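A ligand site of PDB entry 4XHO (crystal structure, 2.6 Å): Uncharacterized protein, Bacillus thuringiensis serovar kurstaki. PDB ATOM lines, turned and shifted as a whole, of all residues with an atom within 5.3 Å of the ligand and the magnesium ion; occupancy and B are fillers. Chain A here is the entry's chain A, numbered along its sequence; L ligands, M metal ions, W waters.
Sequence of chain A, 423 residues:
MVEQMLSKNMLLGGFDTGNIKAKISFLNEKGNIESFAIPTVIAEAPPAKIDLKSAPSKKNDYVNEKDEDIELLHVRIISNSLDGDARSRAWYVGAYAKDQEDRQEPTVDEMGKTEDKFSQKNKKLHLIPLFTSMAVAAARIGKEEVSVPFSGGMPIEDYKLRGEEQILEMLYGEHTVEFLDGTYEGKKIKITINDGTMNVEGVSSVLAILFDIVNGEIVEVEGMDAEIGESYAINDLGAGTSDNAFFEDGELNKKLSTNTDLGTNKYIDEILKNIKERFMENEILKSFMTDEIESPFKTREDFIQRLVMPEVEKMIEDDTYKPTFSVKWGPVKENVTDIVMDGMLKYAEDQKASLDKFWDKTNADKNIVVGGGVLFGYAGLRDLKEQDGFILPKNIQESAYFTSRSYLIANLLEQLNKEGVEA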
ATOM      1  N   ASP A  16      30.016  21.265 -26.311  1.00  0.00           N
ATOM      2  CA  ASP A  16      28.671  20.990 -26.808  1.00  0.00           C
ATOM      3  C   ASP A  16      27.753  20.627 -25.623  1.00  0.00           C
ATOM      4  O   ASP A  16      27.577  19.475 -25.285  1.00  0.00           O
ATOM      5  CB  ASP A  16      28.708  19.866 -27.847  1.00  0.00           C
ATOM      6  CG  ASP A  16      27.329  19.393 -28.301  1.00  0.00           C
ATOM      7  OD1 ASP A  16      26.326  20.129 -28.124  1.00  0.00           O
ATOM      8  OD2 ASP A  16      27.257  18.273 -28.846  1.00  0.00           O
ATOM      9  N   GLY A  18      24.390  20.058 -23.737  1.00  0.00           N
ATOM     10  CA  GLY A  18      22.949  19.870 -23.761  1.00  0.00           C
ATOM     11  C   GLY A  18      22.435  19.535 -22.377  1.00  0.00           C
ATOM     12  O   GLY A  18      23.148  19.687 -21.384  1.00  0.00           O
ATOM     13  N   ASN A  19      21.209  19.056 -22.293  1.00  0.00           N
ATOM     14  CA  ASN A  19      20.639  18.785 -20.980  1.00  0.00           C
ATOM     15  C   ASN A  19      20.718  17.329 -20.567  1.00  0.00           C
ATOM     16  O   ASN A  19      20.512  17.008 -19.403  1.00  0.00           O
ATOM     17  CB  ASN A  19      19.194  19.290 -20.929  1.00  0.00           C
ATOM     18  CG  ASN A  19      19.076  20.712 -21.430  1.00  0.00           C
ATOM     19  OD1 ASN A  19      20.089  21.375 -21.689  1.00  0.00           O
ATOM     20  ND2 ASN A  19      17.850  21.201 -21.545  1.00  0.00           N
ATOM     21  N   ILE A  20      21.021  16.436 -21.512  1.00  0.00           N
ATOM     22  CA  ILE A  20      21.492  15.110 -21.125  1.00  0.00           C
ATOM     23  C   ILE A  20      22.924  15.275 -20.603  1.00  0.00           C
ATOM     24  O   ILE A  20      23.181  15.107 -19.408  1.00  0.00           O
ATOM     25  CB  ILE A  20      21.460  14.082 -22.277  1.00  0.00           C
ATOM     26  CG1 ILE A  20      20.078  14.061 -22.939  1.00  0.00           C
ATOM     27  CG2 ILE A  20      21.788  12.683 -21.761  1.00  0.00           C
ATOM     28  CD1 ILE A  20      19.005  13.690 -21.992  1.00  0.00           C
ATOM     29  N   LYS A  21      23.862  15.643 -21.496  1.00  0.00           N
ATOM     30  CA  LYS A  21      25.258  15.770 -21.086  1.00  0.00           C
ATOM     31  C   LYS A  21      25.983  17.020 -21.555  1.00  0.00           C
ATOM     32  O   LYS A  21      25.533  17.766 -22.437  1.00  0.00           O
ATOM     33  CB  LYS A  21      26.040  14.538 -21.529  1.00  0.00           C
ATOM     34  CG  LYS A  21      25.468  13.772 -22.716  1.00  0.00           C
ATOM     35  CD  LYS A  21      26.128  12.392 -22.836  1.00  0.00           C
ATOM     36  CE  LYS A  21      25.697  11.622 -24.088  1.00  0.00           C
ATOM     37  NZ  LYS A  21      24.254  11.216 -24.093  1.00  0.00           N
ATOM     38  N   LYS A  23      29.256  17.817 -23.417  1.00  0.00           N
ATOM     39  CA  LYS A  23      30.331  17.199 -24.180  1.00  0.00           C
ATOM     40  C   LYS A  23      31.484  18.167 -24.494  1.00  0.00           C
ATOM     41  O   LYS A  23      31.262  19.348 -24.807  1.00  0.00           O
ATOM     42  CB  LYS A  23      29.798  16.626 -25.471  1.00  0.00           C
ATOM     43  CG  LYS A  23      28.590  15.729 -25.271  1.00  0.00           C
ATOM     44  CD  LYS A  23      28.473  14.737 -26.413  1.00  0.00           C
ATOM     45  CE  LYS A  23      27.142  14.860 -27.089  1.00  0.00           C
ATOM     46  NZ  LYS A  23      27.119  14.034 -28.302  1.00  0.00           N
ATOM     47  N   ASP A 236      21.483  16.068 -36.232  1.00  0.00           N
ATOM     48  CA  ASP A 236      22.213  15.565 -35.079  1.00  0.00           C
ATOM     49  C   ASP A 236      21.232  14.710 -34.302  1.00  0.00           C
ATOM     50  O   ASP A 236      20.337  15.225 -33.656  1.00  0.00           O
ATOM     51  CB  ASP A 236      22.783  16.693 -34.232  1.00  0.00           C
ATOM     52  CG  ASP A 236      23.787  16.209 -33.188  1.00  0.00           C
ATOM     53  OD1 ASP A 236      23.593  15.113 -32.627  1.00  0.00           O
ATOM     54  OD2 ASP A 236      24.784  16.920 -32.916  1.00  0.00           O
ATOM     55  N   LEU A 237      21.399  13.387 -34.378  1.00  0.00           N
ATOM     56  CA  LEU A 237      20.524  12.451 -33.691  1.00  0.00           C
ATOM     57  C   LEU A 237      20.997  12.212 -32.244  1.00  0.00           C
ATOM     58  O   LEU A 237      22.043  11.579 -32.001  1.00  0.00           O
ATOM     59  CB  LEU A 237      20.455  11.134 -34.473  1.00  0.00           C
ATOM     60  CG  LEU A 237      20.332  11.251 -36.016  1.00  0.00           C
ATOM     61  CD1 LEU A 237      20.024   9.918 -36.680  1.00  0.00           C
ATOM     62  CD2 LEU A 237      19.313  12.293 -36.439  1.00  0.00           C
ATOM     63  N   GLY A 238      20.246  12.732 -31.280  1.00  0.00           N
ATOM     64  CA  GLY A 238      20.687  12.705 -29.897  1.00  0.00           C
ATOM     65  C   GLY A 238      19.890  11.805 -28.974  1.00  0.00           C
ATOM     66  O   GLY A 238      18.941  11.108 -29.400  1.00  0.00           O
ATOM     67  N   ALA A 239      20.266  11.835 -27.692  1.00  0.00           N
ATOM     68  CA  ALA A 239      19.643  11.017 -26.652  1.00  0.00           C
ATOM     69  C   ALA A 239      18.158  11.348 -26.433  1.00  0.00           C
ATOM     70  O   ALA A 239      17.296  10.473 -26.561  1.00  0.00           O
ATOM     71  CB  ALA A 239      20.397  11.158 -25.353  1.00  0.00           C
ATOM     72  N   GLY A 240      17.853  12.619 -26.141  1.00  0.00           N
ATOM     73  CA  GLY A 240      16.470  13.070 -26.005  1.00  0.00           C
ATOM     74  C   GLY A 240      15.900  13.873 -27.167  1.00  0.00           C
ATOM     75  O   GLY A 240      14.703  14.153 -27.230  1.00  0.00           O
ATOM     76  N   THR A 241      16.754  14.249 -28.107  1.00  0.00           N
ATOM     77  CA  THR A 241      16.344  15.202 -29.142  1.00  0.00           C
ATOM     78  C   THR A 241      16.958  14.858 -30.483  1.00  0.00           C
ATOM     79  O   THR A 241      18.067  14.335 -30.552  1.00  0.00           O
ATOM     80  CB  THR A 241      16.786  16.652 -28.810  1.00  0.00           C
ATOM     81  OG1 THR A 241      18.206  16.784 -29.031  1.00  0.00           O
ATOM     82  CG2 THR A 241      16.472  17.040 -27.364  1.00  0.00           C
ATOM     83  N   THR A 264      16.934   8.762 -28.973  1.00  0.00           N
ATOM     84  CA  THR A 264      17.123   7.381 -28.654  1.00  0.00           C
ATOM     85  C   THR A 264      16.455   6.924 -27.356  1.00  0.00           C
ATOM     86  O   THR A 264      16.040   5.842 -27.234  1.00  0.00           O
ATOM     87  CB  THR A 264      18.602   6.988 -28.627  1.00  0.00           C
ATOM     88  OG1 THR A 264      19.323   7.747 -27.686  1.00  0.00           O
ATOM     89  CG2 THR A 264      19.194   7.161 -29.886  1.00  0.00           C
ATOM     90  N   ASN A 265      16.453   7.752 -26.374  1.00  0.00           N
ATOM     91  CA  ASN A 265      16.143   7.350 -25.001  1.00  0.00           C
ATOM     92  C   ASN A 265      14.849   6.568 -24.868  1.00  0.00           C
ATOM     93  O   ASN A 265      14.788   5.584 -24.131  1.00  0.00           O
ATOM     94  CB  ASN A 265      16.084   8.568 -24.091  1.00  0.00           C
ATOM     95  CG  ASN A 265      17.452   9.011 -23.613  1.00  0.00           C
ATOM     96  OD1 ASN A 265      18.481   8.456 -24.020  1.00  0.00           O
ATOM     97  ND2 ASN A 265      17.472  10.015 -22.744  1.00  0.00           N
ATOM     98  N   ILE A 268      15.469   3.147 -26.187  1.00  0.00           N
ATOM     99  CA  ILE A 268      16.285   2.474 -25.170  1.00  0.00           C
ATOM    100  C   ILE A 268      15.417   2.054 -23.993  1.00  0.00           C
ATOM    101  O   ILE A 268      15.519   0.924 -23.528  1.00  0.00           O
ATOM    102  CB  ILE A 268      17.427   3.381 -24.669  1.00  0.00           C
ATOM    103  CG1 ILE A 268      18.313   3.754 -25.860  1.00  0.00           C
ATOM    104  CG2 ILE A 268      18.176   2.715 -23.505  1.00  0.00           C
ATOM    105  CD1 ILE A 268      19.575   4.477 -25.513  1.00  0.00           C
ATOM    106  N   GLU A 301      23.348   4.795 -19.974  1.00  0.00           N
ATOM    107  CA  GLU A 301      24.721   4.829 -20.466  1.00  0.00           C
ATOM    108  C   GLU A 301      25.444   3.545 -20.120  1.00  0.00           C
ATOM    109  O   GLU A 301      26.335   3.104 -20.850  1.00  0.00           O
ATOM    110  CB  GLU A 301      25.479   6.029 -19.905  1.00  0.00           C
ATOM    111  CG  GLU A 301      25.176   7.319 -20.687  1.00  0.00           C
ATOM    112  CD  GLU A 301      25.693   7.271 -22.135  1.00  0.00           C
ATOM    113  OE1 GLU A 301      26.762   6.652 -22.365  1.00  0.00           O
ATOM    114  OE2 GLU A 301      25.037   7.864 -23.024  1.00  0.00           O
ATOM    115  N   ILE A 304      24.296   1.313 -22.722  1.00  0.00           N
ATOM    116  CA  ILE A 304      24.971   1.648 -23.968  1.00  0.00           C
ATOM    117  C   ILE A 304      26.427   1.209 -23.902  1.00  0.00           C
ATOM    118  O   ILE A 304      26.943   0.583 -24.829  1.00  0.00           O
ATOM    119  CB  ILE A 304      24.870   3.183 -24.285  1.00  0.00           C
ATOM    120  CG1 ILE A 304      23.428   3.549 -24.649  1.00  0.00           C
ATOM    121  CG2 ILE A 304      25.746   3.549 -25.467  1.00  0.00           C
ATOM    122  CD1 ILE A 304      22.909   2.856 -25.904  1.00  0.00           C
ATOM    123  N   VAL A 308      25.853  -2.457 -25.520  1.00  0.00           N
ATOM    124  CA  VAL A 308      25.610  -2.105 -26.906  1.00  0.00           C
ATOM    125  C   VAL A 308      26.853  -1.638 -27.682  1.00  0.00           C
ATOM    126  O   VAL A 308      27.072  -2.109 -28.796  1.00  0.00           O
ATOM    127  CB  VAL A 308      24.520  -1.030 -26.968  1.00  0.00           C
ATOM    128  CG1 VAL A 308      24.375  -0.464 -28.370  1.00  0.00           C
ATOM    129  CG2 VAL A 308      23.201  -1.640 -26.498  1.00  0.00           C
ATOM    130  N   MET A 309      27.649  -0.747 -27.109  1.00  0.00           N
ATOM    131  CA  MET A 309      28.816  -0.220 -27.819  1.00  0.00           C
ATOM    132  C   MET A 309      29.794  -1.263 -28.414  1.00  0.00           C
ATOM    133  O   MET A 309      30.221  -1.110 -29.556  1.00  0.00           O
ATOM    134  CB  MET A 309      29.595   0.720 -26.893  1.00  0.00           C
ATOM    135  CG  MET A 309      28.965   2.092 -26.729  1.00  0.00           C
ATOM    136  SD  MET A 309      29.914   3.146 -25.604  1.00  0.00           S
ATOM    137  CE  MET A 309      29.119   4.750 -25.806  1.00  0.00           C
ATOM    138  N   VAL A 312      28.332  -2.687 -31.615  1.00  0.00           N
ATOM    139  CA  VAL A 312      28.305  -1.690 -32.679  1.00  0.00           C
ATOM    140  C   VAL A 312      29.712  -1.475 -33.240  1.00  0.00           C
ATOM    141  O   VAL A 312      29.886  -1.470 -34.461  1.00  0.00           O
ATOM    142  CB  VAL A 312      27.728  -0.343 -32.191  1.00  0.00           C
ATOM    143  CG1 VAL A 312      28.101   0.766 -33.146  1.00  0.00           C
ATOM    144  CG2 VAL A 312      26.201  -0.439 -32.052  1.00  0.00           C
ATOM    145  N   GLY A 371      25.685  12.439 -34.645  1.00  0.00           N
ATOM    146  CA  GLY A 371      25.164  12.210 -33.302  1.00  0.00           C
ATOM    147  C   GLY A 371      25.239  10.740 -32.892  1.00  0.00           C
ATOM    148  O   GLY A 371      25.557   9.849 -33.691  1.00  0.00           O
ATOM    149  N   GLY A 372      24.941  10.474 -31.638  1.00  0.00           N
ATOM    150  CA  GLY A 372      25.047   9.118 -31.164  1.00  0.00           C
ATOM    151  C   GLY A 372      23.997   8.194 -31.753  1.00  0.00           C
ATOM    152  O   GLY A 372      24.186   6.996 -31.769  1.00  0.00           O
ATOM    153  N   GLY A 373      22.885   8.744 -32.230  1.00  0.00           N
ATOM    154  CA  GLY A 373      21.822   7.931 -32.800  1.00  0.00           C
ATOM    155  C   GLY A 373      22.294   7.125 -33.994  1.00  0.00           C
ATOM    156  O   GLY A 373      21.785   6.044 -34.253  1.00  0.00           O
ATOM    157  N   LEU A 375      25.095   5.661 -34.252  1.00  0.00           N
ATOM    158  CA  LEU A 375      25.750   4.483 -33.722  1.00  0.00           C
ATOM    159  C   LEU A 375      24.732   3.537 -33.097  1.00  0.00           C
ATOM    160  O   LEU A 375      24.743   2.323 -33.348  1.00  0.00           O
ATOM    161  CB  LEU A 375      26.801   4.881 -32.697  1.00  0.00           C
ATOM    162  CG  LEU A 375      27.989   5.639 -33.316  1.00  0.00           C
ATOM    163  CD1 LEU A 375      28.804   6.371 -32.229  1.00  0.00           C
ATOM    164  CD2 LEU A 375      28.869   4.681 -34.130  1.00  0.00           C
ATOM    165  N   PHE A 376      23.825   4.103 -32.291  1.00  0.00           N
ATOM    166  CA  PHE A 376      22.833   3.312 -31.615  1.00  0.00           C
ATOM    167  C   PHE A 376      21.984   2.559 -32.611  1.00  0.00           C
ATOM    168  O   PHE A 376      21.757   1.375 -32.447  1.00  0.00           O
ATOM    169  CB  PHE A 376      21.928   4.167 -30.723  1.00  0.00           C
ATOM    170  CG  PHE A 376      20.700   3.428 -30.239  1.00  0.00           C
ATOM    171  CD1 PHE A 376      20.812   2.430 -29.259  1.00  0.00           C
ATOM    172  CD2 PHE A 376      19.446   3.682 -30.806  1.00  0.00           C
ATOM    173  CE1 PHE A 376      19.693   1.722 -28.827  1.00  0.00           C
ATOM    174  CE2 PHE A 376      18.328   2.973 -30.375  1.00  0.00           C
ATOM    175  CZ  PHE A 376      18.455   1.984 -29.381  1.00  0.00           C
ATOM    176  N   GLN A 397      32.846   6.220 -35.574  1.00  0.00           N
ATOM    177  CA  GLN A 397      32.947   6.056 -34.119  1.00  0.00           C
ATOM    178  C   GLN A 397      32.903   7.408 -33.403  1.00  0.00           C
ATOM    179  O   GLN A 397      32.468   7.484 -32.246  1.00  0.00           O
ATOM    180  CB  GLN A 397      34.214   5.309 -33.686  1.00  0.00           C
ATOM    181  CG  GLN A 397      34.406   3.930 -34.252  1.00  0.00           C
ATOM    182  CD  GLN A 397      35.104   3.964 -35.599  1.00  0.00           C
ATOM    183  OE1 GLN A 397      35.077   4.989 -36.303  1.00  0.00           O
ATOM    184  NE2 GLN A 397      35.755   2.857 -35.960  1.00  0.00           N
ATOM    185  N   ALA A 400      29.100  10.677 -32.235  1.00  0.00           N
ATOM    186  CA  ALA A 400      28.458  11.354 -31.102  1.00  0.00           C
ATOM    187  C   ALA A 400      29.111  12.710 -30.767  1.00  0.00           C
ATOM    188  O   ALA A 400      28.420  13.651 -30.370  1.00  0.00           O
ATOM    189  CB  ALA A 400      28.465  10.461 -29.872  1.00  0.00           C
HETATM  190  P1  LIG L   1      21.019  15.425 -26.864  1.00  0.00           P
HETATM  191  O1  LIG L   1      19.659  15.031 -26.329  1.00  0.00           O
HETATM  192  O2  LIG L   1      21.837  16.318 -25.948  1.00  0.00           O
HETATM  193  O3  LIG L   1      21.018  15.815 -28.333  1.00  0.00           O
HETATM  194  P2  LIG L   1      23.401  13.830 -26.692  1.00  0.00           P
HETATM  195  O4  LIG L   1      23.754  13.711 -25.239  1.00  0.00           O
HETATM  196  O5  LIG L   1      24.118  14.778 -27.641  1.00  0.00           O
HETATM  197  O6  LIG L   1      21.821  14.031 -26.867  1.00  0.00           O
HETATM  198  P3  LIG L   1      24.478  11.634 -28.131  1.00  0.00           P
HETATM  199  O7  LIG L   1      25.823  11.787 -27.440  1.00  0.00           O
HETATM  200  O8  LIG L   1      24.275  12.197 -29.508  1.00  0.00           O
HETATM  201  O9  LIG L   1      23.333  12.309 -27.239  1.00  0.00           O
HETATM  202  O10 LIG L   1      24.006  10.107 -28.135  1.00  0.00           O
HETATM  203  C1  LIG L   1      22.687   9.766 -28.548  1.00  0.00           C
HETATM  204  C2  LIG L   1      22.476   8.283 -28.306  1.00  0.00           C
HETATM  205  O11 LIG L   1      23.489   7.489 -28.940  1.00  0.00           O
HETATM  206  C3  LIG L   1      22.569   8.006 -26.822  1.00  0.00           C
HETATM  207  O12 LIG L   1      21.509   7.116 -26.457  1.00  0.00           O
HETATM  208  C4  LIG L   1      23.920   7.355 -26.650  1.00  0.00           C
HETATM  209  O13 LIG L   1      23.983   6.539 -25.480  1.00  0.00           O
HETATM  210  C5  LIG L   1      24.046   6.604 -27.971  1.00  0.00           C
HETATM  211  N1  LIG L   1      25.436   6.258 -28.344  1.00  0.00           N
HETATM  212  C6  LIG L   1      26.506   7.059 -28.288  1.00  0.00           C
HETATM  213  N2  LIG L   1      27.622   6.421 -28.739  1.00  0.00           N
HETATM  214  C7  LIG L   1      27.258   5.181 -29.076  1.00  0.00           C
HETATM  215  C8  LIG L   1      27.953   3.988 -29.611  1.00  0.00           C
HETATM  216  N3  LIG L   1      29.278   4.018 -29.866  1.00  0.00           N
HETATM  217  N4  LIG L   1      27.217   2.879 -29.824  1.00  0.00           N
HETATM  218  C9  LIG L   1      25.895   2.855 -29.561  1.00  0.00           C
HETATM  219  N5  LIG L   1      25.193   3.889 -29.082  1.00  0.00           N
HETATM  220  C10 LIG L   1      25.819   5.064 -28.818  1.00  0.00           C
HETATM  221 MG    MG M   1      23.103  16.227 -28.763  1.00  0.00          MG
HETATM  222  O   HOH W   1      18.648  16.965 -24.681  1.00  0.00           O
HETATM  223  O   HOH W   2      21.055  16.430 -30.874  1.00  0.00           O
HETATM  224  O   HOH W   3      25.610  16.406 -29.623  1.00  0.00           O
HETATM  225  O   HOH W   4      30.167   1.738 -29.988  1.00  0.00           O
HETATM  226  O   HOH W   5      23.684  14.516 -30.439  1.00  0.00           O
HETATM  227  O   HOH W   6      27.052   9.781 -26.565  1.00  0.00           O
HETATM  228  O   HOH W   7      23.178  18.020 -30.267  1.00  0.00           O
HETATM  229  O   HOH W   8      31.800   5.259 -29.843  1.00  0.00           O
HETATM  230  O   HOH W   9      24.545  17.663 -27.658  1.00  0.00           O
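Water W9 lies within hydrogen-bond range of the side-chain carboxylate of Asp 16 and an oxygen (O2) of the ligand. Water W3 lies within hydrogen-bond range of OD2 of Asp 16, NZ of Lys 23 and OD2 of Asp 236. Water W4 lies within hydrogen-bond range of N3 of the ligand (2.5 Å) and O of Met 309 (2.9 Å). Water W2 bridges O of Asp 236 and OG1 of Thr 241. Water W8 lies within hydrogen-bond range of N3 of the ligand (2.8 Å) and O of Gln 397 (3.3 Å).
The side-chain amino group of Lys 23 lies within salt-bridge range of an oxygen (O7) of the ligand, 2.7 Å away. O13 of the ligand sits at hydrogen-bond distance from OE2 of Glu 301 (3.0 Å). O1 of the ligand sits at hydrogen-bond distance from N of Gly 240, at 3.0 Å. The backbone NH (N) of Phe 376 sits at hydrogen-bond distance from a nitrogen (N5) of the ligand (3.5 Å). An oxygen (O12) of the ligand lies within hydrogen-bond range of the side-chain hydroxyl (OG1) of Thr 264 (2.6 Å). NZ of Lys 21 lies within salt-bridge range of O4 of the ligand (2.8 Å). The backbone NH (N) of Gly 372 is in hydrogen-bond range of an oxygen (O8) of the ligand (2.8 Å). The backbone NH of Thr 241 is in hydrogen-bond range of an oxygen (O1) of the ligand (3.5 Å). N of Ala 239 lies within hydrogen-bond range of O6 of the ligand, 2.8 Å away. An oxygen (O3) of the ligand lies close to the side-chain hydroxyl (OG1) of Thr 241 (3.1 Å).
No residue comes within 4 Å of the magnesium ion. The nearest printed residue that does not touch the magnesium ion is Asp 236 (4.1 Å).
An oxygen (O8) of the ligand sits close to the backbone carbonyl oxygen (O) of Leu 237 (3.4 Å). CG1 of Ile 20 touches O1 of the ligand, at 3.6 Å. C of Gly 238 touches C1 of the ligand, at 3.5 Å. Ile 268 touches the ligand. CG1 of Ile 304 touches O13 of the ligand, 3.2 Å away. Val 308 touches the ligand. Met 309 touches the ligand. C of Gly 371 touches O8 of the ligand, 3.8 Å away. Gly 373 touches the ligand. Leu 375 touches the ligand (CD1 to N3, 3.4 Å). Ala 400 touches the ligand (CB to O7, 3.8 Å). 20 residues have an atom within 4 Å of the ligand: Ile 20, Lys 21, Lys 23, Leu 237, Gly 238, Ala 239, Gly 240, Thr 241, Thr 264, Ile 268, Glu 301, Ile 304, Val 308, Met 309, Gly 371, Gly 372, Gly 373, Leu 375, Phe 376 and Ala 400. The nearest printed residue that does not touch the ligand is Val 312 (4.03 Å).
The backbone NH of Gly 373 sits at hydrogen-bond distance from the backbone carbonyl oxygen of Leu 237 (3.0 Å). The backbone NH of Asn 265 sits at hydrogen-bond distance from the backbone carbonyl oxygen of Ala 239. N of Thr 264 is in hydrogen-bond range of O of Gly 238, at 3.1 Å. O of Ala 239 lies within hydrogen-bond range of N of Thr 264 (3.0 Å). O of Leu 237 sits at hydrogen-bond distance from N of Gly 372. OE2 of Glu 301 lies within salt-bridge range of NZ of Lys 21, 3.6 Å away. O of Ile 304 is in hydrogen-bond range of N of Met 309. NZ of Lys 23 is in hydrogen-bond range of O of Ala 400 (2.5 Å).
The magnesium ion is bound by O5 of the ligand (2.1 Å), O3 of the ligand (2.2 Å), water W9 (2.3 Å), water W7 (2.3 Å) and water W5 (2.5 Å). The magnesium ion has five donor atoms within binding distance. Slightly farther from the magnesium ion lies water W3 (2.7 Å).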
